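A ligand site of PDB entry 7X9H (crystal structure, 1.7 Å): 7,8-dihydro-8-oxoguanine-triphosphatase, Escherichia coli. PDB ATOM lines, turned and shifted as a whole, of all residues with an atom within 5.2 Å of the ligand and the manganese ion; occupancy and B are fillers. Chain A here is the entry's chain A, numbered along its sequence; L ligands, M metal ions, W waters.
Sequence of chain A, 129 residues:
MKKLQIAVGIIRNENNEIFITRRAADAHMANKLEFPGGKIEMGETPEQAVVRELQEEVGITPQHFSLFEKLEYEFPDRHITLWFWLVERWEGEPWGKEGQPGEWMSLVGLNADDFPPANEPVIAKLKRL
Along chain A the residues within 4 Å of the manganese ion span positions 37 to 57.
Ile 6 touches the ligand. Val 8 touches the ligand. Gly 38 touches the ligand (CA to O5, 3.5 Å). OE2 of Glu 53 touches O5 of the ligand, at 3.5 Å. Phe 75 touches the ligand (CZ to O14, 3.4 Å). Ile 80 touches the ligand (CD1 to O11, 3.4 Å). Leu 82 touches the ligand (CD1 to O14, 3.6 Å). Pro 116 touches the ligand (CB to O14, 3.3 Å). CB of Ala 118 touches O14 of the ligand (3.6 Å). Of the 23 residues printed, 17 come within 4 Å of the ligand. The nearest printed residue that does not touch the ligand is Arg 78 (4.2 Å).
The manganese ion is bound by O8 of the ligand (2.1 Å), O6 of the ligand (2.2 Å), O of Gly 37 (2.2 Å), OE2 of Glu 57 (2.2 Å), water W3 (2.2 Å) and water W4 (2.3 Å).
The guanidinium group (NE) of Arg 23 is in hydrogen-bond range of the backbone carbonyl oxygen (O) of His 28 (2.8 Å). NH1 of Arg 23 lies within salt-bridge range of OE1 of Glu 34, at 2.9 Å.
O9 of the ligand is in salt-bridge range of NH2 of Arg 23 (2.9 Å). O of Phe 35 sits at hydrogen-bond distance from N3 of the ligand (2.6 Å). The backbone NH of Phe 35 lies within hydrogen-bond range of an oxygen (O13) of the ligand, at 3.1 Å. N of Lys 39 lies within hydrogen-bond range of O5 of the ligand (3.1 Å). A ring nitrogen (ND1) of His 28 lies within hydrogen-bond range of an oxygen (O12) of the ligand. A nitrogen (N4) of the ligand is in hydrogen-bond range of the side-chain carboxylate (OE1) of Glu 34. A nitrogen (N2) of the ligand sits at hydrogen-bond distance from the side-chain amide oxygen of Asn 119, 2.7 Å away.
Water W3 lies within hydrogen-bond range of the side-chain carboxylate (OE1) of Glu 57 (2.7 Å), the side-chain carboxylate (OE1) of Glu 34 (2.8 Å), a nitrogen (N4) of the ligand (2.9 Å) and the backbone NH (N) of Gly 37 (3.5 Å). Water W1 lies within hydrogen-bond range of O1 of the ligand (2.6 Å) and OE1 of Glu 98 (2.7 Å). Water W2 lies within hydrogen-bond range of NH1 of Arg 78 (2.8 Å) and O12 of the ligand (2.9 Å).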
ATOM      1  N   ILE A   6     -28.718  -8.822  18.969  1.00  0.00           N
ATOM      2  CA  ILE A   6     -28.157  -7.570  18.466  1.00  0.00           C
ATOM      3  C   ILE A   6     -29.271  -6.531  18.329  1.00  0.00           C
ATOM      4  O   ILE A   6     -30.325  -6.833  17.748  1.00  0.00           O
ATOM      5  CB  ILE A   6     -27.463  -7.773  17.103  1.00  0.00           C
ATOM      6  CG1 ILE A   6     -26.376  -8.865  17.164  1.00  0.00           C
ATOM      7  CG2 ILE A   6     -26.918  -6.441  16.616  1.00  0.00           C
ATOM      8  CD1 ILE A   6     -25.265  -8.601  18.137  1.00  0.00           C
ATOM      9  N   VAL A   8     -30.099  -2.739  16.770  1.00  0.00           N
ATOM     10  CA  VAL A   8     -29.601  -1.722  15.846  1.00  0.00           C
ATOM     11  C   VAL A   8     -30.658  -0.649  15.655  1.00  0.00           C
ATOM     12  O   VAL A   8     -31.857  -0.876  15.867  1.00  0.00           O
ATOM     13  CB  VAL A   8     -29.181  -2.331  14.481  1.00  0.00           C
ATOM     14  CG1 VAL A   8     -28.280  -3.523  14.688  1.00  0.00           C
ATOM     15  CG2 VAL A   8     -30.387  -2.683  13.633  1.00  0.00           C
ATOM     16  N   ARG A  23     -18.664  -1.069   8.440  1.00  0.00           N
ATOM     17  CA  ARG A  23     -17.955  -1.920   9.393  1.00  0.00           C
ATOM     18  C   ARG A  23     -16.478  -2.057   9.030  1.00  0.00           C
ATOM     19  O   ARG A  23     -16.102  -2.020   7.865  1.00  0.00           O
ATOM     20  CB  ARG A  23     -18.613  -3.295   9.466  1.00  0.00           C
ATOM     21  CG  ARG A  23     -20.062  -3.181   9.922  1.00  0.00           C
ATOM     22  CD  ARG A  23     -20.763  -4.523  10.041  1.00  0.00           C
ATOM     23  NE  ARG A  23     -20.113  -5.480  10.927  1.00  0.00           N
ATOM     24  CZ  ARG A  23     -20.271  -5.514  12.252  1.00  0.00           C
ATOM     25  NH1 ARG A  23     -21.042  -4.617  12.864  1.00  0.00           N
ATOM     26  NH2 ARG A  23     -19.628  -6.451  12.950  1.00  0.00           N
ATOM     27  N   HIS A  28     -16.552  -9.037  11.900  1.00  0.00           N
ATOM     28  CA  HIS A  28     -17.554  -9.864  11.257  1.00  0.00           C
ATOM     29  C   HIS A  28     -18.365  -8.968  10.333  1.00  0.00           C
ATOM     30  O   HIS A  28     -18.617  -7.802  10.655  1.00  0.00           O
ATOM     31  CB  HIS A  28     -18.455 -10.547  12.300  1.00  0.00           C
ATOM     32  CG  HIS A  28     -19.449 -11.484  11.698  1.00  0.00           C
ATOM     33  ND1 HIS A  28     -20.805 -11.221  11.702  1.00  0.00           N
ATOM     34  CD2 HIS A  28     -19.299 -12.668  11.067  1.00  0.00           C
ATOM     35  CE1 HIS A  28     -21.442 -12.212  11.096  1.00  0.00           C
ATOM     36  NE2 HIS A  28     -20.547 -13.099  10.691  1.00  0.00           N
ATOM     37  N   MET A  29     -18.734  -9.506   9.166  1.00  0.00           N
ATOM     38  CA  MET A  29     -19.390  -8.711   8.123  1.00  0.00           C
ATOM     39  C   MET A  29     -18.532  -7.493   7.779  1.00  0.00           C
ATOM     40  O   MET A  29     -18.994  -6.355   7.725  1.00  0.00           O
ATOM     41  CB  MET A  29     -20.814  -8.321   8.546  1.00  0.00           C
ATOM     42  CG  MET A  29     -21.788  -9.501   8.491  1.00  0.00           C
ATOM     43  SD  MET A  29     -22.009 -10.064   6.779  1.00  0.00           S
ATOM     44  CE  MET A  29     -21.099 -11.621   6.755  1.00  0.00           C
ATOM     45  N   GLU A  34     -24.073  -0.729   7.447  1.00  0.00           N
ATOM     46  CA  GLU A  34     -24.774  -1.242   8.616  1.00  0.00           C
ATOM     47  C   GLU A  34     -25.612  -0.147   9.250  1.00  0.00           C
ATOM     48  O   GLU A  34     -25.285   1.040   9.147  1.00  0.00           O
ATOM     49  CB  GLU A  34     -23.791  -1.791   9.659  1.00  0.00           C
ATOM     50  CG  GLU A  34     -22.720  -0.753  10.037  1.00  0.00           C
ATOM     51  CD  GLU A  34     -22.050  -1.037  11.371  1.00  0.00           C
ATOM     52  OE1 GLU A  34     -22.266  -2.126  11.949  1.00  0.00           O
ATOM     53  OE2 GLU A  34     -21.285  -0.158  11.826  1.00  0.00           O
ATOM     54  N   PHE A  35     -26.680  -0.560   9.945  1.00  0.00           N
ATOM     55  CA  PHE A  35     -27.317   0.314  10.934  1.00  0.00           C
ATOM     56  C   PHE A  35     -26.495   0.278  12.221  1.00  0.00           C
ATOM     57  O   PHE A  35     -26.140  -0.795  12.684  1.00  0.00           O
ATOM     58  CB  PHE A  35     -28.752  -0.170  11.227  1.00  0.00           C
ATOM     59  CG  PHE A  35     -29.598  -0.338   9.996  1.00  0.00           C
ATOM     60  CD1 PHE A  35     -29.846   0.745   9.156  1.00  0.00           C
ATOM     61  CD2 PHE A  35     -30.150  -1.556   9.674  1.00  0.00           C
ATOM     62  CE1 PHE A  35     -30.616   0.605   8.025  1.00  0.00           C
ATOM     63  CE2 PHE A  35     -30.940  -1.706   8.548  1.00  0.00           C
ATOM     64  CZ  PHE A  35     -31.164  -0.635   7.720  1.00  0.00           C
ATOM     65  N   PRO A  36     -26.198   1.425  12.834  1.00  0.00           N
ATOM     66  CA  PRO A  36     -25.425   1.379  14.085  1.00  0.00           C
ATOM     67  C   PRO A  36     -26.131   0.510  15.112  1.00  0.00           C
ATOM     68  O   PRO A  36     -27.355   0.512  15.219  1.00  0.00           O
ATOM     69  CB  PRO A  36     -25.381   2.846  14.526  1.00  0.00           C
ATOM     70  CG  PRO A  36     -25.527   3.626  13.211  1.00  0.00           C
ATOM     71  CD  PRO A  36     -26.518   2.800  12.420  1.00  0.00           C
ATOM     72  N   GLY A  37     -25.350  -0.246  15.871  1.00  0.00           N
ATOM     73  CA  GLY A  37     -25.917  -1.123  16.883  1.00  0.00           C
ATOM     74  C   GLY A  37     -24.894  -2.105  17.413  1.00  0.00           C
ATOM     75  O   GLY A  37     -23.707  -2.011  17.109  1.00  0.00           O
ATOM     76  N   GLY A  38     -25.373  -3.043  18.233  1.00  0.00           N
ATOM     77  CA  GLY A  38     -24.446  -3.972  18.837  1.00  0.00           C
ATOM     78  C   GLY A  38     -25.137  -4.921  19.799  1.00  0.00           C
ATOM     79  O   GLY A  38     -26.365  -4.973  19.883  1.00  0.00           O
ATOM     80  N   LYS A  39     -24.310  -5.657  20.536  1.00  0.00           N
ATOM     81  CA  LYS A  39     -24.790  -6.778  21.339  1.00  0.00           C
ATOM     82  C   LYS A  39     -25.590  -6.304  22.556  1.00  0.00           C
ATOM     83  O   LYS A  39     -25.157  -5.399  23.285  1.00  0.00           O
ATOM     84  CB  LYS A  39     -23.606  -7.629  21.783  1.00  0.00           C
ATOM     85  CG  LYS A  39     -22.779  -8.127  20.610  1.00  0.00           C
ATOM     86  CD  LYS A  39     -21.395  -8.610  21.013  1.00  0.00           C
ATOM     87  CE  LYS A  39     -20.560  -8.895  19.776  1.00  0.00           C
ATOM     88  NZ  LYS A  39     -19.323  -9.667  20.071  1.00  0.00           N
ATOM     89  N   GLU A  53     -26.085   1.583  22.512  1.00  0.00           N
ATOM     90  CA  GLU A  53     -25.258   1.379  21.327  1.00  0.00           C
ATOM     91  C   GLU A  53     -25.216   2.631  20.451  1.00  0.00           C
ATOM     92  O   GLU A  53     -24.167   2.966  19.884  1.00  0.00           O
ATOM     93  CB  GLU A  53     -25.750   0.180  20.530  1.00  0.00           C
ATOM     94  CG  GLU A  53     -25.456  -1.150  21.193  1.00  0.00           C
ATOM     95  CD  GLU A  53     -23.990  -1.540  21.108  1.00  0.00           C
ATOM     96  OE1 GLU A  53     -23.257  -0.981  20.269  1.00  0.00           O
ATOM     97  OE2 GLU A  53     -23.572  -2.432  21.857  1.00  0.00           O
ATOM     98  N   GLU A  57     -21.809   4.473  19.556  1.00  0.00           N
ATOM     99  CA  GLU A  57     -21.289   4.389  18.198  1.00  0.00           C
ATOM    100  C   GLU A  57     -21.410   5.711  17.451  1.00  0.00           C
ATOM    101  O   GLU A  57     -20.511   6.055  16.674  1.00  0.00           O
ATOM    102  CB  GLU A  57     -22.001   3.282  17.419  1.00  0.00           C
ATOM    103  CG  GLU A  57     -21.648   1.898  17.956  1.00  0.00           C
ATOM    104  CD  GLU A  57     -21.789   0.800  16.932  1.00  0.00           C
ATOM    105  OE1 GLU A  57     -22.423   1.035  15.872  1.00  0.00           O
ATOM    106  OE2 GLU A  57     -21.253  -0.298  17.176  1.00  0.00           O
ATOM    107  N   PHE A  75     -25.625 -17.056  10.161  1.00  0.00           N
ATOM    108  CA  PHE A  75     -24.403 -16.812   9.422  1.00  0.00           C
ATOM    109  C   PHE A  75     -23.595 -18.107   9.383  1.00  0.00           C
ATOM    110  O   PHE A  75     -23.927 -19.071  10.079  1.00  0.00           O
ATOM    111  CB  PHE A  75     -23.603 -15.689  10.089  1.00  0.00           C
ATOM    112  CG  PHE A  75     -24.162 -14.330   9.841  1.00  0.00           C
ATOM    113  CD1 PHE A  75     -23.928 -13.680   8.641  1.00  0.00           C
ATOM    114  CD2 PHE A  75     -24.908 -13.671  10.823  1.00  0.00           C
ATOM    115  CE1 PHE A  75     -24.435 -12.399   8.406  1.00  0.00           C
ATOM    116  CE2 PHE A  75     -25.399 -12.399  10.596  1.00  0.00           C
ATOM    117  CZ  PHE A  75     -25.170 -11.762   9.392  1.00  0.00           C
ATOM    118  N   ARG A  78     -22.205 -18.252  13.138  1.00  0.00           N
ATOM    119  CA  ARG A  78     -22.898 -17.705  14.292  1.00  0.00           C
ATOM    120  C   ARG A  78     -24.359 -17.489  13.934  1.00  0.00           C
ATOM    121  O   ARG A  78     -24.705 -17.294  12.777  1.00  0.00           O
ATOM    122  CB  ARG A  78     -22.254 -16.391  14.755  1.00  0.00           C
ATOM    123  CG  ARG A  78     -22.373 -15.242  13.773  1.00  0.00           C
ATOM    124  CD  ARG A  78     -21.416 -14.132  14.185  1.00  0.00           C
ATOM    125  NE  ARG A  78     -20.050 -14.549  13.897  1.00  0.00           N
ATOM    126  CZ  ARG A  78     -18.959 -13.965  14.404  1.00  0.00           C
ATOM    127  NH1 ARG A  78     -19.076 -12.931  15.233  1.00  0.00           N
ATOM    128  NH2 ARG A  78     -17.771 -14.430  14.079  1.00  0.00           N
ATOM    129  N   ILE A  80     -27.634 -15.068  14.916  1.00  0.00           N
ATOM    130  CA  ILE A  80     -27.930 -13.801  15.556  1.00  0.00           C
ATOM    131  C   ILE A  80     -29.407 -13.480  15.418  1.00  0.00           C
ATOM    132  O   ILE A  80     -30.064 -13.820  14.419  1.00  0.00           O
ATOM    133  CB  ILE A  80     -27.072 -12.638  15.005  1.00  0.00           C
ATOM    134  CG1 ILE A  80     -27.629 -12.114  13.699  1.00  0.00           C
ATOM    135  CG2 ILE A  80     -25.608 -13.059  14.843  1.00  0.00           C
ATOM    136  CD1 ILE A  80     -26.937 -10.865  13.276  1.00  0.00           C
ATOM    137  N   LEU A  82     -31.685 -10.174  15.372  1.00  0.00           N
ATOM    138  CA  LEU A  82     -31.531  -8.740  15.134  1.00  0.00           C
ATOM    139  C   LEU A  82     -32.814  -8.011  15.457  1.00  0.00           C
ATOM    140  O   LEU A  82     -33.884  -8.368  14.950  1.00  0.00           O
ATOM    141  CB  LEU A  82     -31.129  -8.453  13.683  1.00  0.00           C
ATOM    142  CG  LEU A  82     -29.662  -8.651  13.350  1.00  0.00           C
ATOM    143  CD1 LEU A  82     -29.568  -9.108  11.909  1.00  0.00           C
ATOM    144  CD2 LEU A  82     -28.843  -7.371  13.549  1.00  0.00           C
ATOM    145  N   PHE A  84     -34.394  -4.521  14.896  1.00  0.00           N
ATOM    146  CA  PHE A  84     -34.257  -3.308  14.085  1.00  0.00           C
ATOM    147  C   PHE A  84     -35.229  -2.269  14.632  1.00  0.00           C
ATOM    148  O   PHE A  84     -36.450  -2.416  14.476  1.00  0.00           O
ATOM    149  CB  PHE A  84     -34.565  -3.591  12.620  1.00  0.00           C
ATOM    150  CG  PHE A  84     -33.590  -4.507  11.949  1.00  0.00           C
ATOM    151  CD1 PHE A  84     -32.520  -3.999  11.248  1.00  0.00           C
ATOM    152  CD2 PHE A  84     -33.773  -5.884  11.982  1.00  0.00           C
ATOM    153  CE1 PHE A  84     -31.616  -4.840  10.602  1.00  0.00           C
ATOM    154  CE2 PHE A  84     -32.866  -6.743  11.336  1.00  0.00           C
ATOM    155  CZ  PHE A  84     -31.793  -6.210  10.656  1.00  0.00           C
ATOM    156  N   GLU A  98     -16.847   6.507  16.974  1.00  0.00           N
ATOM    157  CA  GLU A  98     -15.791   5.516  17.156  1.00  0.00           C
ATOM    158  C   GLU A  98     -14.782   5.524  16.002  1.00  0.00           C
ATOM    159  O   GLU A  98     -14.072   4.532  15.810  1.00  0.00           O
ATOM    160  CB  GLU A  98     -16.423   4.123  17.332  1.00  0.00           C
ATOM    161  CG  GLU A  98     -17.183   3.994  18.651  1.00  0.00           C
ATOM    162  CD  GLU A  98     -17.851   2.641  18.842  1.00  0.00           C
ATOM    163  OE1 GLU A  98     -17.973   1.888  17.846  1.00  0.00           O
ATOM    164  OE2 GLU A  98     -18.268   2.330  19.976  1.00  0.00           O
ATOM    165  N   PHE A 115     -25.117  -4.401   2.495  1.00  0.00           N
ATOM    166  CA  PHE A 115     -25.351  -4.667   3.902  1.00  0.00           C
ATOM    167  C   PHE A 115     -25.227  -6.158   4.166  1.00  0.00           C
ATOM    168  O   PHE A 115     -25.214  -6.966   3.238  1.00  0.00           O
ATOM    169  CB  PHE A 115     -26.769  -4.200   4.296  1.00  0.00           C
ATOM    170  CG  PHE A 115     -26.973  -2.716   4.287  1.00  0.00           C
ATOM    171  CD1 PHE A 115     -27.151  -2.023   3.091  1.00  0.00           C
ATOM    172  CD2 PHE A 115     -27.035  -2.003   5.486  1.00  0.00           C
ATOM    173  CE1 PHE A 115     -27.352  -0.668   3.088  1.00  0.00           C
ATOM    174  CE2 PHE A 115     -27.237  -0.642   5.491  1.00  0.00           C
ATOM    175  CZ  PHE A 115     -27.402   0.024   4.292  1.00  0.00           C
ATOM    176  N   PRO A 116     -25.152  -6.576   5.437  1.00  0.00           N
ATOM    177  CA  PRO A 116     -25.190  -8.011   5.714  1.00  0.00           C
ATOM    178  C   PRO A 116     -26.473  -8.610   5.182  1.00  0.00           C
ATOM    179  O   PRO A 116     -27.523  -7.928   5.134  1.00  0.00           O
ATOM    180  CB  PRO A 116     -25.145  -8.073   7.246  1.00  0.00           C
ATOM    181  CG  PRO A 116     -24.411  -6.819   7.638  1.00  0.00           C
ATOM    182  CD  PRO A 116     -24.973  -5.798   6.669  1.00  0.00           C
ATOM    183  N   ALA A 118     -28.567 -10.508   6.353  1.00  0.00           N
ATOM    184  CA  ALA A 118     -29.655 -10.499   7.311  1.00  0.00           C
ATOM    185  C   ALA A 118     -30.545  -9.281   7.136  1.00  0.00           C
ATOM    186  O   ALA A 118     -31.729  -9.316   7.496  1.00  0.00           O
ATOM    187  CB  ALA A 118     -29.091 -10.532   8.725  1.00  0.00           C
ATOM    188  N   ASN A 119     -29.999  -8.180   6.602  1.00  0.00           N
ATOM    189  CA  ASN A 119     -30.774  -6.956   6.499  1.00  0.00           C
ATOM    190  C   ASN A 119     -31.704  -6.917   5.283  1.00  0.00           C
ATOM    191  O   ASN A 119     -32.470  -5.962   5.150  1.00  0.00           O
ATOM    192  CB  ASN A 119     -29.840  -5.738   6.424  1.00  0.00           C
ATOM    193  CG  ASN A 119     -29.090  -5.518   7.704  1.00  0.00           C
ATOM    194  OD1 ASN A 119     -28.873  -6.444   8.477  1.00  0.00           O
ATOM    195  ND2 ASN A 119     -28.667  -4.273   7.942  1.00  0.00           N
HETATM  196  P1  LIG L   1     -17.923  -4.390  19.590  1.00  0.00           P
HETATM  197  O1  LIG L   1     -18.307  -2.935  19.690  1.00  0.00           O
HETATM  198  O2  LIG L   1     -16.836  -4.653  18.590  1.00  0.00           O
HETATM  199  O3  LIG L   1     -17.712  -5.094  20.907  1.00  0.00           O
HETATM  200  O4  LIG L   1     -19.226  -5.147  19.007  1.00  0.00           O
HETATM  201  P2  LIG L   1     -20.724  -4.530  18.926  1.00  0.00           P
HETATM  202  O5  LIG L   1     -21.385  -4.680  20.273  1.00  0.00           O
HETATM  203  O6  LIG L   1     -20.733  -3.186  18.225  1.00  0.00           O
HETATM  204  O7  LIG L   1     -21.401  -5.644  17.995  1.00  0.00           O
HETATM  205  P3  LIG L   1     -21.447  -5.623  16.395  1.00  0.00           P
HETATM  206  O8  LIG L   1     -22.091  -4.331  15.901  1.00  0.00           O
HETATM  207  O9  LIG L   1     -20.132  -6.060  15.819  1.00  0.00           O
HETATM  208  O10 LIG L   1     -22.464  -6.849  16.206  1.00  0.00           O
HETATM  209  C1  LIG L   1     -23.368  -6.856  15.113  1.00  0.00           C
HETATM  210  C2  LIG L   1     -23.579  -8.285  14.625  1.00  0.00           C
HETATM  211  O11 LIG L   1     -24.811  -8.311  13.924  1.00  0.00           O
HETATM  212  C3  LIG L   1     -22.534  -8.668  13.607  1.00  0.00           C
HETATM  213  O12 LIG L   1     -22.507 -10.100  13.483  1.00  0.00           O
HETATM  214  C4  LIG L   1     -23.088  -8.084  12.333  1.00  0.00           C
HETATM  215  C5  LIG L   1     -24.577  -8.375  12.517  1.00  0.00           C
HETATM  216  N1  LIG L   1     -25.405  -7.380  11.780  1.00  0.00           N
HETATM  217  C6  LIG L   1     -26.242  -7.609  10.742  1.00  0.00           C
HETATM  218  N2  LIG L   1     -26.869  -6.513  10.279  1.00  0.00           N
HETATM  219  C7  LIG L   1     -26.385  -5.491  11.103  1.00  0.00           C
HETATM  220  C8  LIG L   1     -26.626  -4.108  11.161  1.00  0.00           C
HETATM  221  O13 LIG L   1     -27.394  -3.532  10.384  1.00  0.00           O
HETATM  222  N3  LIG L   1     -25.964  -3.355  12.137  1.00  0.00           N
HETATM  223  C9  LIG L   1     -25.101  -3.971  13.028  1.00  0.00           C
HETATM  224  N4  LIG L   1     -24.472  -3.237  13.976  1.00  0.00           N
HETATM  225  N5  LIG L   1     -24.872  -5.291  12.961  1.00  0.00           N
HETATM  226  C10 LIG L   1     -25.496  -6.048  12.029  1.00  0.00           C
HETATM  227  O14 LIG L   1     -26.390  -8.737  10.270  1.00  0.00           O
HETATM  228 MN    MN M   1     -21.645  -2.331  16.467  1.00  0.00          MN
HETATM  229  O   HOH W   1     -18.606  -0.726  18.300  1.00  0.00           O
HETATM  230  O   HOH W   2     -20.944 -10.962  15.784  1.00  0.00           O
HETATM  231  O   HOH W   3     -22.330  -1.350  14.609  1.00  0.00           O
HETATM  232  O   HOH W   4     -19.582  -2.195  15.561  1.00  0.00           O
HETATM  233  O   HOH W   5     -19.224  -8.797  16.043  1.00  0.00           O
HETATM  234  O   HOH W   6     -17.906  -1.746  22.199  1.00  0.00           O
HETATM  235  O   HOH W   7     -17.935  -4.658  15.780  1.00  0.00           O
HETATM  236  O   HOH W   8     -19.243  -4.649  22.846  1.00  0.00           O
